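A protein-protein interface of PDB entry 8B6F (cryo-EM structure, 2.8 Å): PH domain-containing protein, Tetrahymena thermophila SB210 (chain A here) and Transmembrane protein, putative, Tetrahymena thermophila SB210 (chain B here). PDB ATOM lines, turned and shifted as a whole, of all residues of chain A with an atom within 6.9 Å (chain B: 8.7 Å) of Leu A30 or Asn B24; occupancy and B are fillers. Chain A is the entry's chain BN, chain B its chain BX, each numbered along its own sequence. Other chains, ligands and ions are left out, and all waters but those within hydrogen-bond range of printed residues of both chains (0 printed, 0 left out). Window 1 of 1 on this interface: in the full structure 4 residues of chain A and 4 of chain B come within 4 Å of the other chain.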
ATOM      1  N   LYS A  24      25.848  -5.845  39.657  1.00  0.00           N
ATOM      2  CA  LYS A  24      24.893  -4.768  39.418  1.00  0.00           C
ATOM      3  C   LYS A  24      25.319  -3.914  38.231  1.00  0.00           C
ATOM      4  O   LYS A  24      24.486  -3.535  37.399  1.00  0.00           O
ATOM      5  CB  LYS A  24      24.745  -3.909  40.671  1.00  0.00           C
ATOM      6  CG  LYS A  24      24.029  -4.611  41.808  1.00  0.00           C
ATOM      7  CD  LYS A  24      23.983  -3.746  43.057  1.00  0.00           C
ATOM      8  CE  LYS A  24      23.136  -2.497  42.864  1.00  0.00           C
ATOM      9  NZ  LYS A  24      21.735  -2.809  42.470  1.00  0.00           N
ATOM     10  N   VAL A  25      26.611  -3.597  38.136  1.00  0.00           N
ATOM     11  CA  VAL A  25      27.097  -2.810  37.008  1.00  0.00           C
ATOM     12  C   VAL A  25      26.848  -3.552  35.702  1.00  0.00           C
ATOM     13  O   VAL A  25      26.433  -2.956  34.700  1.00  0.00           O
ATOM     14  CB  VAL A  25      28.588  -2.472  37.196  1.00  0.00           C
ATOM     15  CG1 VAL A  25      29.174  -1.862  35.927  1.00  0.00           C
ATOM     16  CG2 VAL A  25      28.768  -1.527  38.366  1.00  0.00           C
ATOM     17  N   ILE A  26      27.110  -4.860  35.685  1.00  0.00           N
ATOM     18  CA  ILE A  26      26.908  -5.638  34.466  1.00  0.00           C
ATOM     19  C   ILE A  26      25.437  -5.646  34.074  1.00  0.00           C
ATOM     20  O   ILE A  26      25.092  -5.462  32.901  1.00  0.00           O
ATOM     21  CB  ILE A  26      27.459  -7.065  34.649  1.00  0.00           C
ATOM     22  CG1 ILE A  26      28.984  -7.032  34.745  1.00  0.00           C
ATOM     23  CG2 ILE A  26      27.026  -7.965  33.498  1.00  0.00           C
ATOM     24  CD1 ILE A  26      29.597  -8.327  35.217  1.00  0.00           C
ATOM     25  N   ASN A  27      24.545  -5.858  35.043  1.00  0.00           N
ATOM     26  CA  ASN A  27      23.120  -5.881  34.730  1.00  0.00           C
ATOM     27  C   ASN A  27      22.653  -4.529  34.213  1.00  0.00           C
ATOM     28  O   ASN A  27      21.889  -4.453  33.244  1.00  0.00           O
ATOM     29  CB  ASN A  27      22.313  -6.290  35.959  1.00  0.00           C
ATOM     30  CG  ASN A  27      22.629  -7.694  36.421  1.00  0.00           C
ATOM     31  OD1 ASN A  27      23.049  -8.538  35.634  1.00  0.00           O
ATOM     32  ND2 ASN A  27      22.425  -7.954  37.706  1.00  0.00           N
ATOM     33  N   TYR A  28      23.098  -3.447  34.853  1.00  0.00           N
ATOM     34  CA  TYR A  28      22.729  -2.113  34.394  1.00  0.00           C
ATOM     35  C   TYR A  28      23.248  -1.860  32.986  1.00  0.00           C
ATOM     36  O   TYR A  28      22.533  -1.307  32.142  1.00  0.00           O
ATOM     37  CB  TYR A  28      23.263  -1.068  35.371  1.00  0.00           C
ATOM     38  CG  TYR A  28      23.226   0.349  34.851  1.00  0.00           C
ATOM     39  CD1 TYR A  28      22.025   1.031  34.719  1.00  0.00           C
ATOM     40  CD2 TYR A  28      24.399   1.012  34.516  1.00  0.00           C
ATOM     41  CE1 TYR A  28      21.991   2.328  34.252  1.00  0.00           C
ATOM     42  CE2 TYR A  28      24.375   2.308  34.049  1.00  0.00           C
ATOM     43  CZ  TYR A  28      23.169   2.960  33.921  1.00  0.00           C
ATOM     44  OH  TYR A  28      23.144   4.253  33.453  1.00  0.00           O
ATOM     45  N   ALA A  29      24.487  -2.264  32.710  1.00  0.00           N
ATOM     46  CA  ALA A  29      25.038  -2.099  31.369  1.00  0.00           C
ATOM     47  C   ALA A  29      24.230  -2.881  30.341  1.00  0.00           C
ATOM     48  O   ALA A  29      23.946  -2.374  29.250  1.00  0.00           O
ATOM     49  CB  ALA A  29      26.501  -2.541  31.348  1.00  0.00           C
ATOM     50  N   LEU A  30      23.847  -4.115  30.673  1.00  0.00           N
ATOM     51  CA  LEU A  30      23.057  -4.914  29.741  1.00  0.00           C
ATOM     52  C   LEU A  30      21.719  -4.252  29.444  1.00  0.00           C
ATOM     53  O   LEU A  30      21.284  -4.208  28.288  1.00  0.00           O
ATOM     54  CB  LEU A  30      22.844  -6.319  30.304  1.00  0.00           C
ATOM     55  CG  LEU A  30      24.085  -7.212  30.393  1.00  0.00           C
ATOM     56  CD1 LEU A  30      23.756  -8.502  31.118  1.00  0.00           C
ATOM     57  CD2 LEU A  30      24.652  -7.509  29.016  1.00  0.00           C
ATOM     58  N   LEU A  31      21.048  -3.736  30.473  1.00  0.00           N
ATOM     59  CA  LEU A  31      19.752  -3.102  30.260  1.00  0.00           C
ATOM     60  C   LEU A  31      19.887  -1.859  29.389  1.00  0.00           C
ATOM     61  O   LEU A  31      19.102  -1.653  28.456  1.00  0.00           O
ATOM     62  CB  LEU A  31      19.121  -2.752  31.607  1.00  0.00           C
ATOM     63  CG  LEU A  31      17.734  -2.110  31.556  1.00  0.00           C
ATOM     64  CD1 LEU A  31      16.742  -2.985  30.809  1.00  0.00           C
ATOM     65  CD2 LEU A  31      17.242  -1.824  32.965  1.00  0.00           C
ATOM     66  N   GLN A  32      20.879  -1.018  29.678  1.00  0.00           N
ATOM     67  CA  GLN A  32      21.072   0.193  28.888  1.00  0.00           C
ATOM     68  C   GLN A  32      21.455  -0.143  27.453  1.00  0.00           C
ATOM     69  O   GLN A  32      21.004   0.520  26.511  1.00  0.00           O
ATOM     70  CB  GLN A  32      22.131   1.082  29.537  1.00  0.00           C
ATOM     71  CG  GLN A  32      21.759   1.554  30.931  1.00  0.00           C
ATOM     72  CD  GLN A  32      20.477   2.360  30.951  1.00  0.00           C
ATOM     73  OE1 GLN A  32      20.174   3.088  30.008  1.00  0.00           O
ATOM     74  NE2 GLN A  32      19.712   2.227  32.024  1.00  0.00           N
ATOM     75  N   ASP A  33      22.282  -1.172  27.266  1.00  0.00           N
ATOM     76  CA  ASP A  33      22.643  -1.598  25.919  1.00  0.00           C
ATOM     77  C   ASP A  33      21.425  -2.095  25.156  1.00  0.00           C
ATOM     78  O   ASP A  33      21.291  -1.842  23.954  1.00  0.00           O
ATOM     79  CB  ASP A  33      23.713  -2.686  25.980  1.00  0.00           C
ATOM     80  CG  ASP A  33      25.014  -2.191  26.571  1.00  0.00           C
ATOM     81  OD1 ASP A  33      25.351  -1.008  26.357  1.00  0.00           O
ATOM     82  OD2 ASP A  33      25.702  -2.982  27.248  1.00  0.00           O
ATOM     83  N   ALA A  34      20.527  -2.809  25.835  1.00  0.00           N
ATOM     84  CA  ALA A  34      19.299  -3.245  25.181  1.00  0.00           C
ATOM     85  C   ALA A  34      18.453  -2.055  24.746  1.00  0.00           C
ATOM     86  O   ALA A  34      17.899  -2.049  23.641  1.00  0.00           O
ATOM     87  CB  ALA A  34      18.504  -4.154  26.112  1.00  0.00           C
ATOM     88  N   LYS A  35      18.333  -1.039  25.603  1.00  0.00           N
ATOM     89  CA  LYS A  35      17.579   0.150  25.222  1.00  0.00           C
ATOM     90  C   LYS A  35      18.205   0.825  24.010  1.00  0.00           C
ATOM     91  O   LYS A  35      17.500   1.214  23.072  1.00  0.00           O
ATOM     92  CB  LYS A  35      17.504   1.124  26.396  1.00  0.00           C
ATOM     93  CG  LYS A  35      16.732   0.603  27.593  1.00  0.00           C
ATOM     94  CD  LYS A  35      16.693   1.639  28.704  1.00  0.00           C
ATOM     95  CE  LYS A  35      15.939   1.129  29.918  1.00  0.00           C
ATOM     96  NZ  LYS A  35      15.971   2.113  31.034  1.00  0.00           N
ATOM     97  N   ARG A  37      20.074  -0.555  21.741  1.00  0.00           N
ATOM     98  CA  ARG A  37      19.828  -1.433  20.606  1.00  0.00           C
ATOM     99  C   ARG A  37      18.434  -1.212  20.041  1.00  0.00           C
ATOM    100  O   ARG A  37      18.252  -1.137  18.821  1.00  0.00           O
ATOM    101  CB  ARG A  37      20.002  -2.883  21.048  1.00  0.00           C
ATOM    102  CG  ARG A  37      20.624  -3.800  20.025  1.00  0.00           C
ATOM    103  CD  ARG A  37      20.737  -5.184  20.619  1.00  0.00           C
ATOM    104  NE  ARG A  37      21.605  -5.197  21.790  1.00  0.00           N
ATOM    105  CZ  ARG A  37      21.546  -6.096  22.762  1.00  0.00           C
ATOM    106  NH1 ARG A  37      20.651  -7.071  22.749  1.00  0.00           N
ATOM    107  NH2 ARG A  37      22.401  -6.012  23.776  1.00  0.00           N
ATOM    108  N   PHE B  21      24.047 -11.694  15.298  1.00  0.00           N
ATOM    109  CA  PHE B  21      22.915 -11.396  16.161  1.00  0.00           C
ATOM    110  C   PHE B  21      23.385 -11.161  17.595  1.00  0.00           C
ATOM    111  O   PHE B  21      24.485 -11.550  17.992  1.00  0.00           O
ATOM    112  CB  PHE B  21      21.898 -12.535  16.124  1.00  0.00           C
ATOM    113  CG  PHE B  21      22.333 -13.758  16.872  1.00  0.00           C
ATOM    114  CD1 PHE B  21      23.236 -14.646  16.311  1.00  0.00           C
ATOM    115  CD2 PHE B  21      21.835 -14.025  18.137  1.00  0.00           C
ATOM    116  CE1 PHE B  21      23.637 -15.775  17.000  1.00  0.00           C
ATOM    117  CE2 PHE B  21      22.232 -15.151  18.830  1.00  0.00           C
ATOM    118  CZ  PHE B  21      23.134 -16.028  18.261  1.00  0.00           C
ATOM    119  N   ALA B  22      22.526 -10.510  18.375  1.00  0.00           N
ATOM    120  CA  ALA B  22      22.834 -10.174  19.758  1.00  0.00           C
ATOM    121  C   ALA B  22      22.407 -11.308  20.679  1.00  0.00           C
ATOM    122  O   ALA B  22      21.275 -11.794  20.596  1.00  0.00           O
ATOM    123  CB  ALA B  22      22.137  -8.878  20.166  1.00  0.00           C
ATOM    124  N   LYS B  23      23.318 -11.724  21.561  1.00  0.00           N
ATOM    125  CA  LYS B  23      23.016 -12.821  22.475  1.00  0.00           C
ATOM    126  C   LYS B  23      22.066 -12.383  23.583  1.00  0.00           C
ATOM    127  O   LYS B  23      21.122 -13.106  23.921  1.00  0.00           O
ATOM    128  CB  LYS B  23      24.311 -13.368  23.075  1.00  0.00           C
ATOM    129  CG  LYS B  23      25.201 -14.107  22.088  1.00  0.00           C
ATOM    130  CD  LYS B  23      24.646 -15.484  21.759  1.00  0.00           C
ATOM    131  CE  LYS B  23      25.617 -16.274  20.899  1.00  0.00           C
ATOM    132  NZ  LYS B  23      25.135 -17.661  20.651  1.00  0.00           N
ATOM    133  N   ASN B  24      22.297 -11.206  24.163  1.00  0.00           N
ATOM    134  CA  ASN B  24      21.531 -10.754  25.325  1.00  0.00           C
ATOM    135  C   ASN B  24      20.169 -10.261  24.860  1.00  0.00           C
ATOM    136  O   ASN B  24      19.988  -9.095  24.508  1.00  0.00           O
ATOM    137  CB  ASN B  24      22.290  -9.666  26.072  1.00  0.00           C
ATOM    138  CG  ASN B  24      23.642 -10.134  26.562  1.00  0.00           C
ATOM    139  OD1 ASN B  24      23.743 -10.815  27.582  1.00  0.00           O
ATOM    140  ND2 ASN B  24      24.693  -9.768  25.839  1.00  0.00           N
ATOM    141  N   ILE B  25      19.193 -11.161  24.869  1.00  0.00           N
ATOM    142  CA  ILE B  25      17.833 -10.822  24.483  1.00  0.00           C
ATOM    143  C   ILE B  25      17.092 -10.264  25.693  1.00  0.00           C
ATOM    144  O   ILE B  25      17.452 -10.510  26.845  1.00  0.00           O
ATOM    145  CB  ILE B  25      17.090 -12.038  23.893  1.00  0.00           C
ATOM    146  CG1 ILE B  25      17.073 -13.197  24.896  1.00  0.00           C
ATOM    147  CG2 ILE B  25      17.740 -12.462  22.586  1.00  0.00           C
ATOM    148  CD1 ILE B  25      16.152 -14.329  24.506  1.00  0.00           C
ATOM    149  N   THR B  26      16.035  -9.498  25.420  1.00  0.00           N
ATOM    150  CA  THR B  26      15.217  -8.901  26.465  1.00  0.00           C
ATOM    151  C   THR B  26      13.820  -9.494  26.560  1.00  0.00           C
ATOM    152  O   THR B  26      13.094  -9.170  27.505  1.00  0.00           O
ATOM    153  CB  THR B  26      15.093  -7.386  26.248  1.00  0.00           C
ATOM    154  OG1 THR B  26      14.726  -7.120  24.889  1.00  0.00           O
ATOM    155  CG2 THR B  26      16.399  -6.696  26.567  1.00  0.00           C
ATOM    156  N   THR B  27      13.420 -10.343  25.611  1.00  0.00           N
ATOM    157  CA  THR B  27      12.099 -10.955  25.689  1.00  0.00           C
ATOM    158  C   THR B  27      11.952 -11.799  26.946  1.00  0.00           C
ATOM    159  O   THR B  27      10.859 -11.877  27.516  1.00  0.00           O
ATOM    160  CB  THR B  27      11.837 -11.805  24.446  1.00  0.00           C
ATOM    161  OG1 THR B  27      12.874 -12.783  24.301  1.00  0.00           O
ATOM    162  CG2 THR B  27      11.790 -10.931  23.203  1.00  0.00           C
ATOM    163  N   THR B  28      13.031 -12.437  27.390  1.00  0.00           N
ATOM    164  CA  THR B  28      13.003 -13.234  28.606  1.00  0.00           C
ATOM    165  C   THR B  28      14.420 -13.355  29.142  1.00  0.00           C
ATOM    166  O   THR B  28      15.394 -13.079  28.438  1.00  0.00           O
ATOM    167  CB  THR B  28      12.402 -14.622  28.356  1.00  0.00           C
ATOM    168  OG1 THR B  28      12.379 -15.366  29.581  1.00  0.00           O
ATOM    169  CG2 THR B  28      13.214 -15.388  27.318  1.00  0.00           C
ATOM    170  N   ASP B  29      14.521 -13.774  30.400  1.00  0.00           N
ATOM    171  CA  ASP B  29      15.808 -13.973  31.049  1.00  0.00           C
ATOM    172  C   ASP B  29      16.291 -15.394  30.791  1.00  0.00           C
ATOM    173  O   ASP B  29      15.539 -16.356  30.974  1.00  0.00           O
ATOM    174  CB  ASP B  29      15.708 -13.708  32.552  1.00  0.00           C
ATOM    175  CG  ASP B  29      14.702 -14.609  33.239  1.00  0.00           C
ATOM    176  OD1 ASP B  29      13.733 -15.033  32.576  1.00  0.00           O
ATOM    177  OD2 ASP B  29      14.878 -14.889  34.442  1.00  0.00           O
ATOM    178  N   ILE B  30      17.540 -15.519  30.365  1.00  0.00           N
ATOM    179  CA  ILE B  30      18.092 -16.832  30.020  1.00  0.00           C
ATOM    180  C   ILE B  30      18.171 -17.690  31.280  1.00  0.00           C
ATOM    181  O   ILE B  30      18.681 -17.219  32.310  1.00  0.00           O
ATOM    182  CB  ILE B  30      19.475 -16.677  29.380  1.00  0.00           C
ATOM    183  CG1 ILE B  30      19.406 -15.737  28.172  1.00  0.00           C
ATOM    184  CG2 ILE B  30      20.019 -18.039  28.964  1.00  0.00           C
ATOM    185  CD1 ILE B  30      20.750 -15.437  27.539  1.00  0.00           C
ATOM    186  N   LYS B  32      19.870 -20.093  33.821  1.00  0.00           N
ATOM    187  CA  LYS B  32      21.293 -20.230  34.079  1.00  0.00           C
ATOM    188  C   LYS B  32      21.510 -20.804  35.469  1.00  0.00           C
ATOM    189  O   LYS B  32      20.650 -20.711  36.347  1.00  0.00           O
ATOM    190  CB  LYS B  32      22.016 -18.886  33.941  1.00  0.00           C
ATOM    191  CG  LYS B  32      21.532 -17.827  34.914  1.00  0.00           C
ATOM    192  CD  LYS B  32      22.339 -16.548  34.788  1.00  0.00           C
ATOM    193  CE  LYS B  32      21.904 -15.515  35.817  1.00  0.00           C
ATOM    194  NZ  LYS B  32      22.071 -15.999  37.216  1.00  0.00           N
ATOM    195  N   TYR B  54      33.099 -14.726  33.776  1.00  0.00           N
ATOM    196  CA  TYR B  54      31.750 -15.245  33.579  1.00  0.00           C
ATOM    197  C   TYR B  54      31.786 -16.763  33.683  1.00  0.00           C
ATOM    198  O   TYR B  54      32.502 -17.423  32.923  1.00  0.00           O
ATOM    199  CB  TYR B  54      31.193 -14.803  32.226  1.00  0.00           C
ATOM    200  CG  TYR B  54      31.253 -13.308  32.019  1.00  0.00           C
ATOM    201  CD1 TYR B  54      32.385 -12.707  31.483  1.00  0.00           C
ATOM    202  CD2 TYR B  54      30.184 -12.496  32.372  1.00  0.00           C
ATOM    203  CE1 TYR B  54      32.446 -11.340  31.297  1.00  0.00           C
ATOM    204  CE2 TYR B  54      30.236 -11.129  32.189  1.00  0.00           C
ATOM    205  CZ  TYR B  54      31.370 -10.558  31.654  1.00  0.00           C
ATOM    206  OH  TYR B  54      31.428  -9.198  31.470  1.00  0.00           O
ATOM    207  N   TYR B  58      24.293 -22.962  31.103  1.00  0.00           N
ATOM    208  CA  TYR B  58      22.891 -23.148  30.761  1.00  0.00           C
ATOM    209  C   TYR B  58      22.265 -24.209  31.656  1.00  0.00           C
ATOM    210  O   TYR B  58      22.872 -25.246  31.933  1.00  0.00           O
ATOM    211  CB  TYR B  58      22.746 -23.554  29.294  1.00  0.00           C
ATOM    212  CG  TYR B  58      23.054 -22.446  28.316  1.00  0.00           C
ATOM    213  CD1 TYR B  58      22.112 -21.470  28.024  1.00  0.00           C
ATOM    214  CD2 TYR B  58      24.284 -22.381  27.677  1.00  0.00           C
ATOM    215  CE1 TYR B  58      22.389 -20.456  27.127  1.00  0.00           C
ATOM    216  CE2 TYR B  58      24.570 -21.373  26.780  1.00  0.00           C
ATOM    217  CZ  TYR B  58      23.619 -20.414  26.508  1.00  0.00           C
ATOM    218  OH  TYR B  58      23.902 -19.407  25.616  1.00  0.00           O
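O of Asn B24 lies within hydrogen-bond range of NH1 of Arg A37.
Of the printed residues of chain B, Leu A30 touches Asn B24 (3.7 Å). Asn B24 touches just these residues of chain A: Leu A30 (3.7 Å) and Arg A37 (2.8 Å). No residue of chain B comes within 4 Å of Ala A29. Printed residues of chain A within 4 Å of Thr B26: Ala A34 (3.3 Å). Of the printed residues of chain A, Ala B22 touches Arg A37. Of the printed residues of chain B, Arg A37 touches Ala B22 (3.5 Å) and Asn B24 (2.8 Å). Asp B29 touches none of the printed residues of chain A. Thr B28 touches none of the printed residues of chain A.
Of the 13 printed residues of chain B, 3 touch a printed residue of chain A. Hydrophobic or aromatic side chains of chain B within 4 Å of the printed part of chain A: Ala B22. Along chain B the printed residues that touch a printed residue of chain A span positions 22 to 26. Of the 13 printed residues of chain A, 3 touch a printed residue of chain B. Printed residues of chain A that touch a printed residue of chain B: Leu A30, Ala A34 and Arg A37. Hydrophobic or aromatic side chains of chain A within 4 Å of the printed part of chain B: Leu A30 and Ala A34. Along chain A the printed residues that touch a printed residue of chain B span positions 30 to 37. Among the printed residues, 4 pairs touch across the chains. Among the printed residues, no Asp or Glu carboxylate lies within 4 Å of a Lys or Arg side-chain nitrogen of the other chain.
CD2 of Leu A30 touches OD1 of Asn B24, 3.7 Å away. Thr B26 touches Ala A34 (CG2 to CB, 3.3 Å). Ala B22 touches Arg A37 (CB to NH1, 3.5 Å).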
